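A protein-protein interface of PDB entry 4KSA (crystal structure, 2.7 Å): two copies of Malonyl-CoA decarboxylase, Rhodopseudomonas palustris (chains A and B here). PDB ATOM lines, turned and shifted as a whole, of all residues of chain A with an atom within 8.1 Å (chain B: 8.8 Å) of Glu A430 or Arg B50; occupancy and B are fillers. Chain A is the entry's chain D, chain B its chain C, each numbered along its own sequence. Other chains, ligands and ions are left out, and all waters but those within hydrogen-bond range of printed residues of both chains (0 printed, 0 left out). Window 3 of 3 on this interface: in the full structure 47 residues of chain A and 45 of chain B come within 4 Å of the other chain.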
ATOM      1  N   ASN A 282      -6.254  11.960 -15.996  1.00  0.00           N
ATOM      2  CA  ASN A 282      -7.579  11.555 -15.546  1.00  0.00           C
ATOM      3  C   ASN A 282      -7.628  11.108 -14.092  1.00  0.00           C
ATOM      4  O   ASN A 282      -8.689  10.766 -13.578  1.00  0.00           O
ATOM      5  CB  ASN A 282      -8.101  10.456 -16.456  1.00  0.00           C
ATOM      6  CG  ASN A 282      -8.190  10.909 -17.884  1.00  0.00           C
ATOM      7  OD1 ASN A 282      -9.055  11.704 -18.238  1.00  0.00           O
ATOM      8  ND2 ASN A 282      -7.270  10.433 -18.714  1.00  0.00           N
ATOM      9  N   ARG A 374     -18.451  10.779 -26.745  1.00  0.00           N
ATOM     10  CA  ARG A 374     -18.289  10.876 -25.299  1.00  0.00           C
ATOM     11  C   ARG A 374     -19.552  11.467 -24.672  1.00  0.00           C
ATOM     12  O   ARG A 374     -20.406  12.007 -25.376  1.00  0.00           O
ATOM     13  CB  ARG A 374     -17.087  11.765 -24.942  1.00  0.00           C
ATOM     14  CG  ARG A 374     -15.726  11.150 -25.234  1.00  0.00           C
ATOM     15  CD  ARG A 374     -14.611  11.854 -24.449  1.00  0.00           C
ATOM     16  NE  ARG A 374     -14.751  11.703 -22.997  1.00  0.00           N
ATOM     17  CZ  ARG A 374     -14.669  10.546 -22.338  1.00  0.00           C
ATOM     18  NH1 ARG A 374     -14.813  10.527 -21.020  1.00  0.00           N
ATOM     19  NH2 ARG A 374     -14.437   9.408 -22.986  1.00  0.00           N
ATOM     20  N   ALA A 423     -10.853   0.992 -12.412  1.00  0.00           N
ATOM     21  CA  ALA A 423     -11.756   0.187 -13.227  1.00  0.00           C
ATOM     22  C   ALA A 423     -12.759   1.040 -14.009  1.00  0.00           C
ATOM     23  O   ALA A 423     -12.922   0.863 -15.226  1.00  0.00           O
ATOM     24  CB  ALA A 423     -12.482  -0.788 -12.360  1.00  0.00           C
ATOM     25  N   ASN A 424     -13.426   1.967 -13.319  1.00  0.00           N
ATOM     26  CA  ASN A 424     -14.410   2.820 -13.984  1.00  0.00           C
ATOM     27  C   ASN A 424     -13.750   3.602 -15.094  1.00  0.00           C
ATOM     28  O   ASN A 424     -14.296   3.716 -16.189  1.00  0.00           O
ATOM     29  CB  ASN A 424     -15.076   3.789 -12.999  1.00  0.00           C
ATOM     30  CG  ASN A 424     -15.874   3.073 -11.924  1.00  0.00           C
ATOM     31  OD1 ASN A 424     -16.628   2.154 -12.214  1.00  0.00           O
ATOM     32  ND2 ASN A 424     -15.713   3.500 -10.676  1.00  0.00           N
ATOM     33  N   HIS A 425     -12.568   4.141 -14.812  1.00  0.00           N
ATOM     34  CA  HIS A 425     -11.833   4.901 -15.817  1.00  0.00           C
ATOM     35  C   HIS A 425     -11.489   3.990 -16.988  1.00  0.00           C
ATOM     36  O   HIS A 425     -11.782   4.312 -18.141  1.00  0.00           O
ATOM     37  CB  HIS A 425     -10.532   5.465 -15.246  1.00  0.00           C
ATOM     38  CG  HIS A 425      -9.596   5.965 -16.302  1.00  0.00           C
ATOM     39  ND1 HIS A 425      -9.801   7.154 -16.967  1.00  0.00           N
ATOM     40  CD2 HIS A 425      -8.548   5.365 -16.915  1.00  0.00           C
ATOM     41  CE1 HIS A 425      -8.926   7.259 -17.951  1.00  0.00           C
ATOM     42  NE2 HIS A 425      -8.158   6.185 -17.941  1.00  0.00           N
ATOM     43  N   GLU A 426     -10.867   2.853 -16.688  1.00  0.00           N
ATOM     44  CA  GLU A 426     -10.479   1.917 -17.733  1.00  0.00           C
ATOM     45  C   GLU A 426     -11.674   1.461 -18.554  1.00  0.00           C
ATOM     46  O   GLU A 426     -11.636   1.507 -19.789  1.00  0.00           O
ATOM     47  CB  GLU A 426      -9.753   0.700 -17.130  1.00  0.00           C
ATOM     48  CG  GLU A 426      -8.297   0.970 -16.763  1.00  0.00           C
ATOM     49  CD  GLU A 426      -7.479   1.512 -17.948  1.00  0.00           C
ATOM     50  OE1 GLU A 426      -6.579   2.352 -17.716  1.00  0.00           O
ATOM     51  OE2 GLU A 426      -7.730   1.093 -19.106  1.00  0.00           O
ATOM     52  N   ALA A 427     -12.735   1.041 -17.858  1.00  0.00           N
ATOM     53  CA  ALA A 427     -13.956   0.557 -18.498  1.00  0.00           C
ATOM     54  C   ALA A 427     -14.597   1.636 -19.340  1.00  0.00           C
ATOM     55  O   ALA A 427     -15.152   1.352 -20.397  1.00  0.00           O
ATOM     56  CB  ALA A 427     -14.932   0.077 -17.453  1.00  0.00           C
ATOM     57  N   LEU A 428     -14.534   2.876 -18.868  1.00  0.00           N
ATOM     58  CA  LEU A 428     -15.106   3.975 -19.632  1.00  0.00           C
ATOM     59  C   LEU A 428     -14.249   4.280 -20.852  1.00  0.00           C
ATOM     60  O   LEU A 428     -14.770   4.402 -21.957  1.00  0.00           O
ATOM     61  CB  LEU A 428     -15.216   5.248 -18.793  1.00  0.00           C
ATOM     62  CG  LEU A 428     -15.424   6.472 -19.694  1.00  0.00           C
ATOM     63  CD1 LEU A 428     -16.707   6.303 -20.479  1.00  0.00           C
ATOM     64  CD2 LEU A 428     -15.441   7.746 -18.878  1.00  0.00           C
ATOM     65  N   PHE A 429     -12.939   4.414 -20.649  1.00  0.00           N
ATOM     66  CA  PHE A 429     -12.031   4.734 -21.750  1.00  0.00           C
ATOM     67  C   PHE A 429     -11.829   3.601 -22.764  1.00  0.00           C
ATOM     68  O   PHE A 429     -11.826   3.846 -23.975  1.00  0.00           O
ATOM     69  CB  PHE A 429     -10.681   5.208 -21.194  1.00  0.00           C
ATOM     70  CG  PHE A 429     -10.584   6.698 -21.044  1.00  0.00           C
ATOM     71  CD1 PHE A 429     -11.620   7.420 -20.471  1.00  0.00           C
ATOM     72  CD2 PHE A 429      -9.474   7.389 -21.507  1.00  0.00           C
ATOM     73  CE1 PHE A 429     -11.554   8.806 -20.369  1.00  0.00           C
ATOM     74  CE2 PHE A 429      -9.402   8.778 -21.408  1.00  0.00           C
ATOM     75  CZ  PHE A 429     -10.442   9.485 -20.840  1.00  0.00           C
ATOM     76  N   GLU A 430     -11.672   2.370 -22.283  1.00  0.00           N
ATOM     77  CA  GLU A 430     -11.485   1.246 -23.184  1.00  0.00           C
ATOM     78  C   GLU A 430     -12.770   0.834 -23.910  1.00  0.00           C
ATOM     79  O   GLU A 430     -12.721   0.462 -25.080  1.00  0.00           O
ATOM     80  CB  GLU A 430     -10.922   0.047 -22.431  1.00  0.00           C
ATOM     81  CG  GLU A 430      -9.457   0.168 -22.066  1.00  0.00           C
ATOM     82  CD  GLU A 430      -8.564   0.257 -23.290  1.00  0.00           C
ATOM     83  OE1 GLU A 430      -8.795  -0.525 -24.236  1.00  0.00           O
ATOM     84  OE2 GLU A 430      -7.631   1.090 -23.310  1.00  0.00           O
ATOM     85  N   ARG A 431     -13.918   0.916 -23.239  1.00  0.00           N
ATOM     86  CA  ARG A 431     -15.172   0.508 -23.864  1.00  0.00           C
ATOM     87  C   ARG A 431     -16.336   1.492 -23.897  1.00  0.00           C
ATOM     88  O   ARG A 431     -17.466   1.078 -24.135  1.00  0.00           O
ATOM     89  CB  ARG A 431     -15.659  -0.792 -23.234  1.00  0.00           C
ATOM     90  CG  ARG A 431     -14.742  -1.947 -23.513  1.00  0.00           C
ATOM     91  CD  ARG A 431     -13.941  -2.283 -22.294  1.00  0.00           C
ATOM     92  NE  ARG A 431     -14.833  -2.669 -21.211  1.00  0.00           N
ATOM     93  CZ  ARG A 431     -14.442  -2.929 -19.965  1.00  0.00           C
ATOM     94  NH1 ARG A 431     -15.350  -3.275 -19.053  1.00  0.00           N
ATOM     95  NH2 ARG A 431     -13.154  -2.841 -19.626  1.00  0.00           N
ATOM     96  N   GLY A 432     -16.076   2.778 -23.679  1.00  0.00           N
ATOM     97  CA  GLY A 432     -17.153   3.768 -23.701  1.00  0.00           C
ATOM     98  C   GLY A 432     -18.293   3.502 -22.718  1.00  0.00           C
ATOM     99  O   GLY A 432     -19.345   4.134 -22.788  1.00  0.00           O
ATOM    100  N   GLN A 433     -18.062   2.575 -21.794  1.00  0.00           N
ATOM    101  CA  GLN A 433     -19.032   2.176 -20.787  1.00  0.00           C
ATOM    102  C   GLN A 433     -19.161   3.127 -19.602  1.00  0.00           C
ATOM    103  O   GLN A 433     -18.256   3.222 -18.777  1.00  0.00           O
ATOM    104  CB  GLN A 433     -18.661   0.784 -20.285  1.00  0.00           C
ATOM    105  CG  GLN A 433     -19.458   0.306 -19.101  1.00  0.00           C
ATOM    106  CD  GLN A 433     -19.272  -1.180 -18.861  1.00  0.00           C
ATOM    107  OE1 GLN A 433     -18.144  -1.659 -18.687  1.00  0.00           O
ATOM    108  NE2 GLN A 433     -20.382  -1.923 -18.850  1.00  0.00           N
ATOM    109  N   THR B  45       0.554  -2.905 -28.608  1.00  0.00           N
ATOM    110  CA  THR B  45      -0.530  -2.850 -27.646  1.00  0.00           C
ATOM    111  C   THR B  45      -0.617  -1.482 -26.983  1.00  0.00           C
ATOM    112  O   THR B  45      -1.698  -0.910 -26.884  1.00  0.00           O
ATOM    113  CB  THR B  45      -0.350  -3.893 -26.574  1.00  0.00           C
ATOM    114  OG1 THR B  45      -0.500  -5.179 -27.167  1.00  0.00           O
ATOM    115  CG2 THR B  45      -1.380  -3.707 -25.464  1.00  0.00           C
ATOM    116  N   LEU B  46       0.523  -0.968 -26.531  1.00  0.00           N
ATOM    117  CA  LEU B  46       0.583   0.331 -25.889  1.00  0.00           C
ATOM    118  C   LEU B  46       0.184   1.480 -26.814  1.00  0.00           C
ATOM    119  O   LEU B  46      -0.363   2.482 -26.362  1.00  0.00           O
ATOM    120  CB  LEU B  46       1.983   0.570 -25.338  1.00  0.00           C
ATOM    121  CG  LEU B  46       2.268   1.946 -24.731  1.00  0.00           C
ATOM    122  CD1 LEU B  46       1.179   2.332 -23.738  1.00  0.00           C
ATOM    123  CD2 LEU B  46       3.643   1.919 -24.057  1.00  0.00           C
ATOM    124  N   LEU B  47       0.434   1.339 -28.108  1.00  0.00           N
ATOM    125  CA  LEU B  47       0.080   2.406 -29.046  1.00  0.00           C
ATOM    126  C   LEU B  47      -1.415   2.487 -29.365  1.00  0.00           C
ATOM    127  O   LEU B  47      -1.898   3.480 -29.937  1.00  0.00           O
ATOM    128  CB  LEU B  47       0.839   2.234 -30.359  1.00  0.00           C
ATOM    129  CG  LEU B  47       2.283   2.703 -30.414  1.00  0.00           C
ATOM    130  CD1 LEU B  47       2.897   2.276 -31.743  1.00  0.00           C
ATOM    131  CD2 LEU B  47       2.337   4.207 -30.254  1.00  0.00           C
ATOM    132  N   SER B  48      -2.143   1.440 -29.001  1.00  0.00           N
ATOM    133  CA  SER B  48      -3.562   1.377 -29.294  1.00  0.00           C
ATOM    134  C   SER B  48      -4.393   1.436 -28.025  1.00  0.00           C
ATOM    135  O   SER B  48      -5.619   1.355 -28.069  1.00  0.00           O
ATOM    136  CB  SER B  48      -3.860   0.081 -30.023  1.00  0.00           C
ATOM    137  OG  SER B  48      -3.726  -0.987 -29.104  1.00  0.00           O
ATOM    138  N   ARG B  49      -3.715   1.565 -26.893  1.00  0.00           N
ATOM    139  CA  ARG B  49      -4.380   1.632 -25.609  1.00  0.00           C
ATOM    140  C   ARG B  49      -5.053   2.996 -25.415  1.00  0.00           C
ATOM    141  O   ARG B  49      -4.535   4.025 -25.866  1.00  0.00           O
ATOM    142  CB  ARG B  49      -3.352   1.391 -24.515  1.00  0.00           C
ATOM    143  CG  ARG B  49      -3.930   0.815 -23.263  1.00  0.00           C
ATOM    144  CD  ARG B  49      -4.472  -0.552 -23.547  1.00  0.00           C
ATOM    145  NE  ARG B  49      -5.164  -1.099 -22.391  1.00  0.00           N
ATOM    146  CZ  ARG B  49      -5.925  -2.185 -22.432  1.00  0.00           C
ATOM    147  NH1 ARG B  49      -6.088  -2.833 -23.575  1.00  0.00           N
ATOM    148  NH2 ARG B  49      -6.523  -2.620 -21.336  1.00  0.00           N
ATOM    149  N   ARG B  50      -6.214   3.009 -24.761  1.00  0.00           N
ATOM    150  CA  ARG B  50      -6.922   4.267 -24.513  1.00  0.00           C
ATOM    151  C   ARG B  50      -6.882   4.645 -23.032  1.00  0.00           C
ATOM    152  O   ARG B  50      -6.656   5.802 -22.672  1.00  0.00           O
ATOM    153  CB  ARG B  50      -8.369   4.165 -24.983  1.00  0.00           C
ATOM    154  CG  ARG B  50      -8.508   3.821 -26.446  1.00  0.00           C
ATOM    155  CD  ARG B  50      -9.965   3.837 -26.852  1.00  0.00           C
ATOM    156  NE  ARG B  50     -10.335   2.713 -27.717  1.00  0.00           N
ATOM    157  CZ  ARG B  50     -10.156   1.426 -27.411  1.00  0.00           C
ATOM    158  NH1 ARG B  50     -10.536   0.473 -28.263  1.00  0.00           N
ATOM    159  NH2 ARG B  50      -9.574   1.088 -26.264  1.00  0.00           N
ATOM    160  N   GLY B  51      -7.101   3.652 -22.178  1.00  0.00           N
ATOM    161  CA  GLY B  51      -7.075   3.883 -20.752  1.00  0.00           C
ATOM    162  C   GLY B  51      -5.734   4.438 -20.331  1.00  0.00           C
ATOM    163  O   GLY B  51      -4.710   4.131 -20.938  1.00  0.00           O
ATOM    164  N   GLU B  52      -5.742   5.261 -19.290  1.00  0.00           N
ATOM    165  CA  GLU B  52      -4.530   5.868 -18.777  1.00  0.00           C
ATOM    166  C   GLU B  52      -3.829   4.972 -17.761  1.00  0.00           C
ATOM    167  O   GLU B  52      -2.612   4.965 -17.677  1.00  0.00           O
ATOM    168  CB  GLU B  52      -4.856   7.242 -18.171  1.00  0.00           C
ATOM    169  CG  GLU B  52      -3.753   7.851 -17.312  1.00  0.00           C
ATOM    170  CD  GLU B  52      -4.052   9.290 -16.911  1.00  0.00           C
ATOM    171  OE1 GLU B  52      -3.383   9.813 -15.991  1.00  0.00           O
ATOM    172  OE2 GLU B  52      -4.949   9.908 -17.529  1.00  0.00           O
ATOM    173  N   ALA B  53      -4.598   4.213 -16.996  1.00  0.00           N
ATOM    174  CA  ALA B  53      -4.027   3.324 -16.000  1.00  0.00           C
ATOM    175  C   ALA B  53      -3.333   2.160 -16.684  1.00  0.00           C
ATOM    176  O   ALA B  53      -2.183   1.844 -16.361  1.00  0.00           O
ATOM    177  CB  ALA B  53      -5.101   2.805 -15.077  1.00  0.00           C
ATOM    178  N   SER B  54      -4.027   1.518 -17.623  1.00  0.00           N
ATOM    179  CA  SER B  54      -3.462   0.386 -18.360  1.00  0.00           C
ATOM    180  C   SER B  54      -2.303   0.863 -19.262  1.00  0.00           C
ATOM    181  O   SER B  54      -1.390   0.092 -19.611  1.00  0.00           O
ATOM    182  CB  SER B  54      -4.553  -0.286 -19.203  1.00  0.00           C
ATOM    183  OG  SER B  54      -5.083   0.605 -20.180  1.00  0.00           O
ATOM    184  N   GLY B  55      -2.341   2.143 -19.627  1.00  0.00           N
ATOM    185  CA  GLY B  55      -1.292   2.708 -20.448  1.00  0.00           C
ATOM    186  C   GLY B  55       0.035   2.731 -19.714  1.00  0.00           C
ATOM    187  O   GLY B  55       1.024   2.213 -20.223  1.00  0.00           O
ATOM    188  N   VAL B  56       0.070   3.310 -18.514  1.00  0.00           N
ATOM    189  CA  VAL B  56       1.324   3.382 -17.774  1.00  0.00           C
ATOM    190  C   VAL B  56       1.754   1.972 -17.392  1.00  0.00           C
ATOM    191  O   VAL B  56       2.943   1.674 -17.277  1.00  0.00           O
ATOM    192  CB  VAL B  56       1.204   4.263 -16.479  1.00  0.00           C
ATOM    193  CG1 VAL B  56       0.532   5.586 -16.797  1.00  0.00           C
ATOM    194  CG2 VAL B  56       0.439   3.520 -15.423  1.00  0.00           C
ATOM    195  N   LEU B  58       1.254  -0.822 -19.183  1.00  0.00           N
ATOM    196  CA  LEU B  58       1.913  -1.456 -20.316  1.00  0.00           C
ATOM    197  C   LEU B  58       3.284  -0.816 -20.532  1.00  0.00           C
ATOM    198  O   LEU B  58       4.250  -1.495 -20.897  1.00  0.00           O
ATOM    199  CB  LEU B  58       1.057  -1.315 -21.580  1.00  0.00           C
ATOM    200  CG  LEU B  58      -0.234  -2.145 -21.599  1.00  0.00           C
ATOM    201  CD1 LEU B  58      -1.075  -1.769 -22.801  1.00  0.00           C
ATOM    202  CD2 LEU B  58       0.101  -3.629 -21.632  1.00  0.00           C
ATOM    203  N   ARG B 125       4.607   7.871 -24.890  1.00  0.00           N
ATOM    204  CA  ARG B 125       3.857   7.062 -23.942  1.00  0.00           C
ATOM    205  C   ARG B 125       4.759   6.346 -22.941  1.00  0.00           C
ATOM    206  O   ARG B 125       4.451   6.297 -21.752  1.00  0.00           O
ATOM    207  CB  ARG B 125       2.972   6.062 -24.671  1.00  0.00           C
ATOM    208  CG  ARG B 125       1.906   6.758 -25.462  1.00  0.00           C
ATOM    209  CD  ARG B 125       0.916   5.809 -26.061  1.00  0.00           C
ATOM    210  NE  ARG B 125      -0.150   6.547 -26.722  1.00  0.00           N
ATOM    211  CZ  ARG B 125      -1.370   6.059 -26.922  1.00  0.00           C
ATOM    212  NH1 ARG B 125      -1.670   4.821 -26.513  1.00  0.00           N
ATOM    213  NH2 ARG B 125      -2.305   6.819 -27.487  1.00  0.00           N
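NE of Arg B49 sits at hydrogen-bond distance from OG of Ser B54 (2.8 Å).
O of Arg B49 is in hydrogen-bond range of NH1 of Arg B125 (3.0 Å).
Printed residues of chain B within 4 Å of Asn A282: Glu B52 (2.7 Å).
Of chain A, only Glu A430 (3.4 Å) comes within 4 Å of Arg B49.
Printed residues of chain A within 4 Å of Arg B50: Phe A429 and Glu A430.
Of the printed residues of chain A, Ala B53 touches Glu A426 (2.8 Å).
Of the printed residues of chain A, Ser B54 touches Glu A426.
The nearest residue of chain B that does not touch Glu A430 is Ser B54 (4.1 Å).
The nearest residue of chain A that does not touch Arg B50 is His A425 (5.0 Å).
The nearest printed residue of chain B that does not touch Phe A429 is Glu B52 (4.8 Å).
Of the 14 printed residues of chain B, 6 touch a printed residue of chain A.
Printed residues of chain B that touch a printed residue of chain A: Arg B49, Arg B50, Gly B51, Glu B52, Ala B53 and Ser B54.
The backbone NH of Ser B54 sits at hydrogen-bond distance from the side-chain carboxylate of Glu A426 (2.7 Å).
OE2 of Glu B52 is in hydrogen-bond range of ND2 of Asn A282, 2.7 Å away.
The backbone NH of Ala B53 sits at hydrogen-bond distance from the side-chain carboxylate of Glu A426 (2.8 Å).
OE2 of Glu A430 lies within salt-bridge range of NE of Arg B49.
NE2 of His A425 is in hydrogen-bond range of N of Glu B52 (2.9 Å).
The backbone NH (N) of Gly B51 lies within hydrogen-bond range of the side-chain carboxylate (OE2) of Glu A430 (2.9 Å).
The backbone NH (N) of Glu B52 lies within hydrogen-bond range of the side-chain carboxylate (OE1) of Glu A426, at 3.4 Å.
The side-chain carboxylate (OE1) of Glu A430 lies within salt-bridge range of the guanidinium group (NH2) of Arg B50 (2.7 Å).
No position is printed for both chains.
Of the 12 pairs that touch across the chains among the printed residues, none has its exchanged pair printed and touching as well.
Gly B51 touches His A425 (CA to NE2, 3.8 Å).
OE2 of Glu A426 touches CA of Gly B51, 3.3 Å away.
Arg B50 touches Phe A429 (CD to O, 3.4 Å).
Gly B51 touches Phe A429.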
